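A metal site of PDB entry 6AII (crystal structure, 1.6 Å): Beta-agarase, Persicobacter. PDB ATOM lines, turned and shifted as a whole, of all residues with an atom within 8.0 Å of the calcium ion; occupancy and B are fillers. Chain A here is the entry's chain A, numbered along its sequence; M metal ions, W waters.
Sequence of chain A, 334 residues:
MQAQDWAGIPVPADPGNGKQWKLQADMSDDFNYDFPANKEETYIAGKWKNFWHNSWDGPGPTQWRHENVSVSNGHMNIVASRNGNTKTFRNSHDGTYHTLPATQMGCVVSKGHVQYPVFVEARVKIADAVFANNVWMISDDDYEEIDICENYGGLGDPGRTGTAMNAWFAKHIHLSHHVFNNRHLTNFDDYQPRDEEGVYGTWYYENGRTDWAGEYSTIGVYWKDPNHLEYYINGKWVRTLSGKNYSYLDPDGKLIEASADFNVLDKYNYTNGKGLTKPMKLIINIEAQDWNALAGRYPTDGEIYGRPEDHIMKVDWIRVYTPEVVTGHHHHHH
OD2 of Asp 316 is in salt-bridge range of NH2 of Arg 123 (2.7 Å).
Five residues have an atom within 4 Å of the calcium ion: Asp 5, Asp 30, Asn 32, Gly 74 and Asp 316.
The backbone carbonyl oxygen (O) of Gly 74 is bound to the calcium ion, at 2.2 Å. The calcium ion is bound by OD2 of Asp 5, 2.3 Å away. The side-chain carboxylate (OD1) of Asp 316 is bound to the calcium ion. The calcium ion is bound by O of Asp 30 (2.3 Å). The calcium ion is bound by water W1, at 2.5 Å. The side-chain amide oxygen (OD1) of Asn 32 binds the calcium ion (2.5 Å). The calcium ion is bound by O of Asp 316 (2.6 Å).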
ATOM      1  N   GLN A   4     -15.420  15.694  22.324  1.00  0.00           N
ATOM      2  CA  GLN A   4     -14.360  16.764  22.343  1.00  0.00           C
ATOM      3  C   GLN A   4     -14.930  18.029  21.722  1.00  0.00           C
ATOM      4  O   GLN A   4     -16.010  18.043  21.122  1.00  0.00           O
ATOM      5  CB  GLN A   4     -13.179  16.172  21.570  1.00  0.00           C
ATOM      6  CG  GLN A   4     -12.753  14.888  22.293  1.00  0.00           C
ATOM      7  CD  GLN A   4     -11.357  14.417  22.066  1.00  0.00           C
ATOM      8  OE1 GLN A   4     -10.410  14.803  22.771  1.00  0.00           O
ATOM      9  NE2 GLN A   4     -11.252  13.493  21.142  1.00  0.00           N
ATOM     10  N   ASP A   5     -14.137  19.115  21.847  1.00  0.00           N
ATOM     11  CA  ASP A   5     -14.639  20.406  21.416  1.00  0.00           C
ATOM     12  C   ASP A   5     -14.961  20.416  19.918  1.00  0.00           C
ATOM     13  O   ASP A   5     -15.789  21.179  19.477  1.00  0.00           O
ATOM     14  CB  ASP A   5     -13.644  21.527  21.704  1.00  0.00           C
ATOM     15  CG  ASP A   5     -13.521  21.963  23.149  1.00  0.00           C
ATOM     16  OD1 ASP A   5     -14.351  21.561  24.005  1.00  0.00           O
ATOM     17  OD2 ASP A   5     -12.570  22.686  23.410  1.00  0.00           O
ATOM     18  N   TRP A   6     -14.219  19.671  19.114  1.00  0.00           N
ATOM     19  CA  TRP A   6     -14.402  19.656  17.666  1.00  0.00           C
ATOM     20  C   TRP A   6     -15.482  18.654  17.247  1.00  0.00           C
ATOM     21  O   TRP A   6     -15.679  18.439  16.071  1.00  0.00           O
ATOM     22  CB  TRP A   6     -13.072  19.304  16.960  1.00  0.00           C
ATOM     23  CG  TRP A   6     -12.466  18.050  17.490  1.00  0.00           C
ATOM     24  CD1 TRP A   6     -12.858  16.782  17.254  1.00  0.00           C
ATOM     25  CD2 TRP A   6     -11.314  17.959  18.333  1.00  0.00           C
ATOM     26  NE1 TRP A   6     -12.025  15.891  17.852  1.00  0.00           N
ATOM     27  CE2 TRP A   6     -11.095  16.590  18.575  1.00  0.00           C
ATOM     28  CE3 TRP A   6     -10.477  18.909  18.937  1.00  0.00           C
ATOM     29  CZ2 TRP A   6     -10.043  16.154  19.351  1.00  0.00           C
ATOM     30  CZ3 TRP A   6      -9.436  18.464  19.713  1.00  0.00           C
ATOM     31  CH2 TRP A   6      -9.225  17.096  19.910  1.00  0.00           C
ATOM     32  N   ASP A  29      -5.595  18.040  21.027  1.00  0.00           N
ATOM     33  CA  ASP A  29      -5.857  18.526  22.371  1.00  0.00           C
ATOM     34  C   ASP A  29      -6.905  19.617  22.294  1.00  0.00           C
ATOM     35  O   ASP A  29      -6.750  20.520  21.433  1.00  0.00           O
ATOM     36  CB  ASP A  29      -4.575  19.041  23.015  1.00  0.00           C
ATOM     37  CG  ASP A  29      -4.631  19.243  24.513  1.00  0.00           C
ATOM     38  OD1 ASP A  29      -5.741  19.338  25.090  1.00  0.00           O
ATOM     39  OD2 ASP A  29      -3.520  19.210  25.104  1.00  0.00           O
ATOM     40  N   ASP A  30      -7.962  19.565  23.152  1.00  0.00           N
ATOM     41  CA  ASP A  30      -8.906  20.691  23.206  1.00  0.00           C
ATOM     42  C   ASP A  30      -8.755  21.610  24.425  1.00  0.00           C
ATOM     43  O   ASP A  30      -9.583  22.478  24.626  1.00  0.00           O
ATOM     44  CB  ASP A  30     -10.331  20.191  22.996  1.00  0.00           C
ATOM     45  CG  ASP A  30     -10.835  19.155  23.968  1.00  0.00           C
ATOM     46  OD1 ASP A  30     -10.105  18.753  24.875  1.00  0.00           O
ATOM     47  OD2 ASP A  30     -12.020  18.792  23.780  1.00  0.00           O
ATOM     48  N   PHE A  31      -7.649  21.438  25.165  1.00  0.00           N
ATOM     49  CA  PHE A  31      -7.166  22.454  26.118  1.00  0.00           C
ATOM     50  C   PHE A  31      -8.198  22.861  27.184  1.00  0.00           C
ATOM     51  O   PHE A  31      -8.349  24.048  27.505  1.00  0.00           O
ATOM     52  CB  PHE A  31      -6.692  23.699  25.321  1.00  0.00           C
ATOM     53  CG  PHE A  31      -5.475  23.396  24.511  1.00  0.00           C
ATOM     54  CD1 PHE A  31      -4.332  22.968  25.145  1.00  0.00           C
ATOM     55  CD2 PHE A  31      -5.463  23.485  23.128  1.00  0.00           C
ATOM     56  CE1 PHE A  31      -3.182  22.684  24.442  1.00  0.00           C
ATOM     57  CE2 PHE A  31      -4.309  23.209  22.414  1.00  0.00           C
ATOM     58  CZ  PHE A  31      -3.180  22.800  23.070  1.00  0.00           C
ATOM     59  N   ASN A  32      -8.886  21.866  27.729  1.00  0.00           N
ATOM     60  CA  ASN A  32      -9.967  22.161  28.690  1.00  0.00           C
ATOM     61  C   ASN A  32      -9.499  21.805  30.101  1.00  0.00           C
ATOM     62  O   ASN A  32     -10.296  21.406  30.953  1.00  0.00           O
ATOM     63  CB  ASN A  32     -11.273  21.522  28.238  1.00  0.00           C
ATOM     64  CG  ASN A  32     -11.757  22.032  26.883  1.00  0.00           C
ATOM     65  OD1 ASN A  32     -11.595  23.223  26.492  1.00  0.00           O
ATOM     66  ND2 ASN A  32     -12.444  21.151  26.174  1.00  0.00           N
ATOM     67  N   TYR A  33      -8.209  21.949  30.337  1.00  0.00           N
ATOM     68  CA  TYR A  33      -7.588  21.746  31.640  1.00  0.00           C
ATOM     69  C   TYR A  33      -6.810  23.021  31.993  1.00  0.00           C
ATOM     70  O   TYR A  33      -6.583  23.884  31.117  1.00  0.00           O
ATOM     71  CB  TYR A  33      -6.660  20.533  31.641  1.00  0.00           C
ATOM     72  CG  TYR A  33      -5.668  20.555  30.499  1.00  0.00           C
ATOM     73  CD1 TYR A  33      -4.485  21.259  30.582  1.00  0.00           C
ATOM     74  CD2 TYR A  33      -5.970  19.991  29.277  1.00  0.00           C
ATOM     75  CE1 TYR A  33      -3.568  21.300  29.536  1.00  0.00           C
ATOM     76  CE2 TYR A  33      -5.072  20.022  28.218  1.00  0.00           C
ATOM     77  CZ  TYR A  33      -3.868  20.709  28.333  1.00  0.00           C
ATOM     78  OH  TYR A  33      -2.987  20.741  27.303  1.00  0.00           O
ATOM     79  N   VAL A  71      -2.521  27.459  29.979  1.00  0.00           N
ATOM     80  CA  VAL A  71      -3.803  26.894  29.509  1.00  0.00           C
ATOM     81  C   VAL A  71      -4.841  27.202  30.551  1.00  0.00           C
ATOM     82  O   VAL A  71      -4.668  26.907  31.728  1.00  0.00           O
ATOM     83  CB  VAL A  71      -3.747  25.393  29.199  1.00  0.00           C
ATOM     84  CG1 VAL A  71      -5.082  24.951  28.595  1.00  0.00           C
ATOM     85  CG2 VAL A  71      -2.614  25.001  28.269  1.00  0.00           C
ATOM     86  N   SER A  72      -5.916  27.837  30.116  1.00  0.00           N
ATOM     87  CA  SER A  72      -7.003  28.249  31.039  1.00  0.00           C
ATOM     88  C   SER A  72      -8.231  28.590  30.210  1.00  0.00           C
ATOM     89  O   SER A  72      -8.143  28.959  29.027  1.00  0.00           O
ATOM     90  CB  SER A  72      -6.673  29.429  31.941  1.00  0.00           C
ATOM     91  OG  SER A  72      -6.480  30.592  31.180  1.00  0.00           O
ATOM     92  N   ASN A  73      -9.395  28.446  30.837  1.00  0.00           N
ATOM     93  CA  ASN A  73     -10.617  28.996  30.287  1.00  0.00           C
ATOM     94  C   ASN A  73     -10.990  28.349  28.936  1.00  0.00           C
ATOM     95  O   ASN A  73     -11.789  28.978  28.201  1.00  0.00           O
ATOM     96  CB  ASN A  73     -10.601  30.508  30.247  1.00  0.00           C
ATOM     97  CG  ASN A  73     -10.336  31.086  31.617  1.00  0.00           C
ATOM     98  OD1 ASN A  73      -9.271  31.675  31.816  1.00  0.00           O
ATOM     99  ND2 ASN A  73     -11.189  30.776  32.567  1.00  0.00           N
ATOM    100  N   GLY A  74     -10.510  27.167  28.677  1.00  0.00           N
ATOM    101  CA  GLY A  74     -10.822  26.374  27.459  1.00  0.00           C
ATOM    102  C   GLY A  74      -9.829  26.517  26.334  1.00  0.00           C
ATOM    103  O   GLY A  74     -10.029  25.870  25.278  1.00  0.00           O
ATOM    104  N   HIS A  75      -8.743  27.270  26.573  1.00  0.00           N
ATOM    105  CA  HIS A  75      -7.753  27.452  25.478  1.00  0.00           C
ATOM    106  C   HIS A  75      -6.343  27.573  26.036  1.00  0.00           C
ATOM    107  O   HIS A  75      -6.100  28.050  27.165  1.00  0.00           O
ATOM    108  CB  HIS A  75      -8.076  28.714  24.668  1.00  0.00           C
ATOM    109  CG  HIS A  75      -8.617  29.809  25.474  1.00  0.00           C
ATOM    110  ND1 HIS A  75      -7.772  30.650  26.231  1.00  0.00           N
ATOM    111  CD2 HIS A  75      -9.873  30.242  25.701  1.00  0.00           C
ATOM    112  CE1 HIS A  75      -8.566  31.529  26.864  1.00  0.00           C
ATOM    113  NE2 HIS A  75      -9.793  31.310  26.548  1.00  0.00           N
ATOM    114  N   MET A  76      -5.407  27.225  25.166  1.00  0.00           N
ATOM    115  CA  MET A  76      -3.997  27.541  25.387  1.00  0.00           C
ATOM    116  C   MET A  76      -3.856  29.051  25.150  1.00  0.00           C
ATOM    117  O   MET A  76      -4.472  29.583  24.187  1.00  0.00           O
ATOM    118  CB  MET A  76      -3.081  26.786  24.433  1.00  0.00           C
ATOM    119  CG  MET A  76      -1.659  27.231  24.510  1.00  0.00           C
ATOM    120  SD  MET A  76      -0.581  26.058  23.570  1.00  0.00           S
ATOM    121  CE  MET A  76      -0.410  24.727  24.645  1.00  0.00           C
ATOM    122  N   ARG A 123      -8.019  25.673  15.909  1.00  0.00           N
ATOM    123  CA  ARG A 123      -9.004  26.686  16.105  1.00  0.00           C
ATOM    124  C   ARG A 123      -8.380  27.725  17.009  1.00  0.00           C
ATOM    125  O   ARG A 123      -8.094  27.417  18.183  1.00  0.00           O
ATOM    126  CB  ARG A 123     -10.300  26.121  16.713  1.00  0.00           C
ATOM    127  CG  ARG A 123     -11.433  27.123  16.795  1.00  0.00           C
ATOM    128  CD  ARG A 123     -12.795  26.531  17.086  1.00  0.00           C
ATOM    129  NE  ARG A 123     -13.848  27.531  16.940  1.00  0.00           N
ATOM    130  CZ  ARG A 123     -14.512  28.131  17.933  1.00  0.00           C
ATOM    131  NH1 ARG A 123     -15.515  28.966  17.635  1.00  0.00           N
ATOM    132  NH2 ARG A 123     -14.230  27.914  19.207  1.00  0.00           N
ATOM    133  N   TYR A 216     -12.949  33.355  16.756  1.00  0.00           N
ATOM    134  CA  TYR A 216     -12.139  32.187  16.439  1.00  0.00           C
ATOM    135  C   TYR A 216     -12.180  31.891  14.948  1.00  0.00           C
ATOM    136  O   TYR A 216     -13.207  32.098  14.280  1.00  0.00           O
ATOM    137  CB  TYR A 216     -12.629  30.964  17.226  1.00  0.00           C
ATOM    138  CG  TYR A 216     -12.171  30.996  18.666  1.00  0.00           C
ATOM    139  CD1 TYR A 216     -12.894  31.629  19.658  1.00  0.00           C
ATOM    140  CD2 TYR A 216     -10.965  30.446  19.041  1.00  0.00           C
ATOM    141  CE1 TYR A 216     -12.451  31.635  20.986  1.00  0.00           C
ATOM    142  CE2 TYR A 216     -10.492  30.495  20.352  1.00  0.00           C
ATOM    143  CZ  TYR A 216     -11.233  31.105  21.325  1.00  0.00           C
ATOM    144  OH  TYR A 216     -10.706  31.127  22.613  1.00  0.00           O
ATOM    145  N   VAL A 315      -5.678  29.326  21.684  1.00  0.00           N
ATOM    146  CA  VAL A 315      -5.855  28.140  20.872  1.00  0.00           C
ATOM    147  C   VAL A 315      -6.942  27.297  21.580  1.00  0.00           C
ATOM    148  O   VAL A 315      -6.680  26.709  22.631  1.00  0.00           O
ATOM    149  CB  VAL A 315      -4.564  27.331  20.682  1.00  0.00           C
ATOM    150  CG1 VAL A 315      -4.792  26.142  19.742  1.00  0.00           C
ATOM    151  CG2 VAL A 315      -3.410  28.212  20.170  1.00  0.00           C
ATOM    152  N   ASP A 316      -8.131  27.244  20.965  1.00  0.00           N
ATOM    153  CA  ASP A 316      -9.234  26.449  21.559  1.00  0.00           C
ATOM    154  C   ASP A 316      -8.938  24.977  21.422  1.00  0.00           C
ATOM    155  O   ASP A 316      -9.272  24.176  22.297  1.00  0.00           O
ATOM    156  CB  ASP A 316     -10.529  26.835  20.850  1.00  0.00           C
ATOM    157  CG  ASP A 316     -11.778  26.180  21.432  1.00  0.00           C
ATOM    158  OD1 ASP A 316     -11.747  25.791  22.627  1.00  0.00           O
ATOM    159  OD2 ASP A 316     -12.773  26.102  20.665  1.00  0.00           O
ATOM    160  N   TRP A 317      -8.407  24.563  20.277  1.00  0.00           N
ATOM    161  CA  TRP A 317      -8.084  23.162  20.071  1.00  0.00           C
ATOM    162  C   TRP A 317      -7.117  23.014  18.901  1.00  0.00           C
ATOM    163  O   TRP A 317      -7.028  23.888  18.002  1.00  0.00           O
ATOM    164  CB  TRP A 317      -9.341  22.283  19.864  1.00  0.00           C
ATOM    165  CG  TRP A 317     -10.393  22.684  18.874  1.00  0.00           C
ATOM    166  CD1 TRP A 317     -11.601  23.183  19.231  1.00  0.00           C
ATOM    167  CD2 TRP A 317     -10.417  22.570  17.449  1.00  0.00           C
ATOM    168  NE1 TRP A 317     -12.424  23.316  18.150  1.00  0.00           N
ATOM    169  CE2 TRP A 317     -11.722  22.942  17.042  1.00  0.00           C
ATOM    170  CE3 TRP A 317      -9.478  22.144  16.486  1.00  0.00           C
ATOM    171  CZ2 TRP A 317     -12.101  22.944  15.716  1.00  0.00           C
ATOM    172  CZ3 TRP A 317      -9.849  22.185  15.149  1.00  0.00           C
ATOM    173  CH2 TRP A 317     -11.150  22.564  14.773  1.00  0.00           C
ATOM    174  N   ILE A 318      -6.411  21.903  18.885  1.00  0.00           N
ATOM    175  CA  ILE A 318      -5.613  21.421  17.800  1.00  0.00           C
ATOM    176  C   ILE A 318      -6.120  19.999  17.531  1.00  0.00           C
ATOM    177  O   ILE A 318      -6.207  19.219  18.509  1.00  0.00           O
ATOM    178  CB  ILE A 318      -4.107  21.386  18.117  1.00  0.00           C
ATOM    179  CG1 ILE A 318      -3.583  22.773  18.464  1.00  0.00           C
ATOM    180  CG2 ILE A 318      -3.332  20.706  17.023  1.00  0.00           C
ATOM    181  CD1 ILE A 318      -2.249  22.743  19.158  1.00  0.00           C
HETATM  182 CA    CA M   1     -11.087  24.226  24.225  1.00  0.00          CA
HETATM  183  O   HOH W   1     -13.249  25.198  25.069  1.00  0.00           O
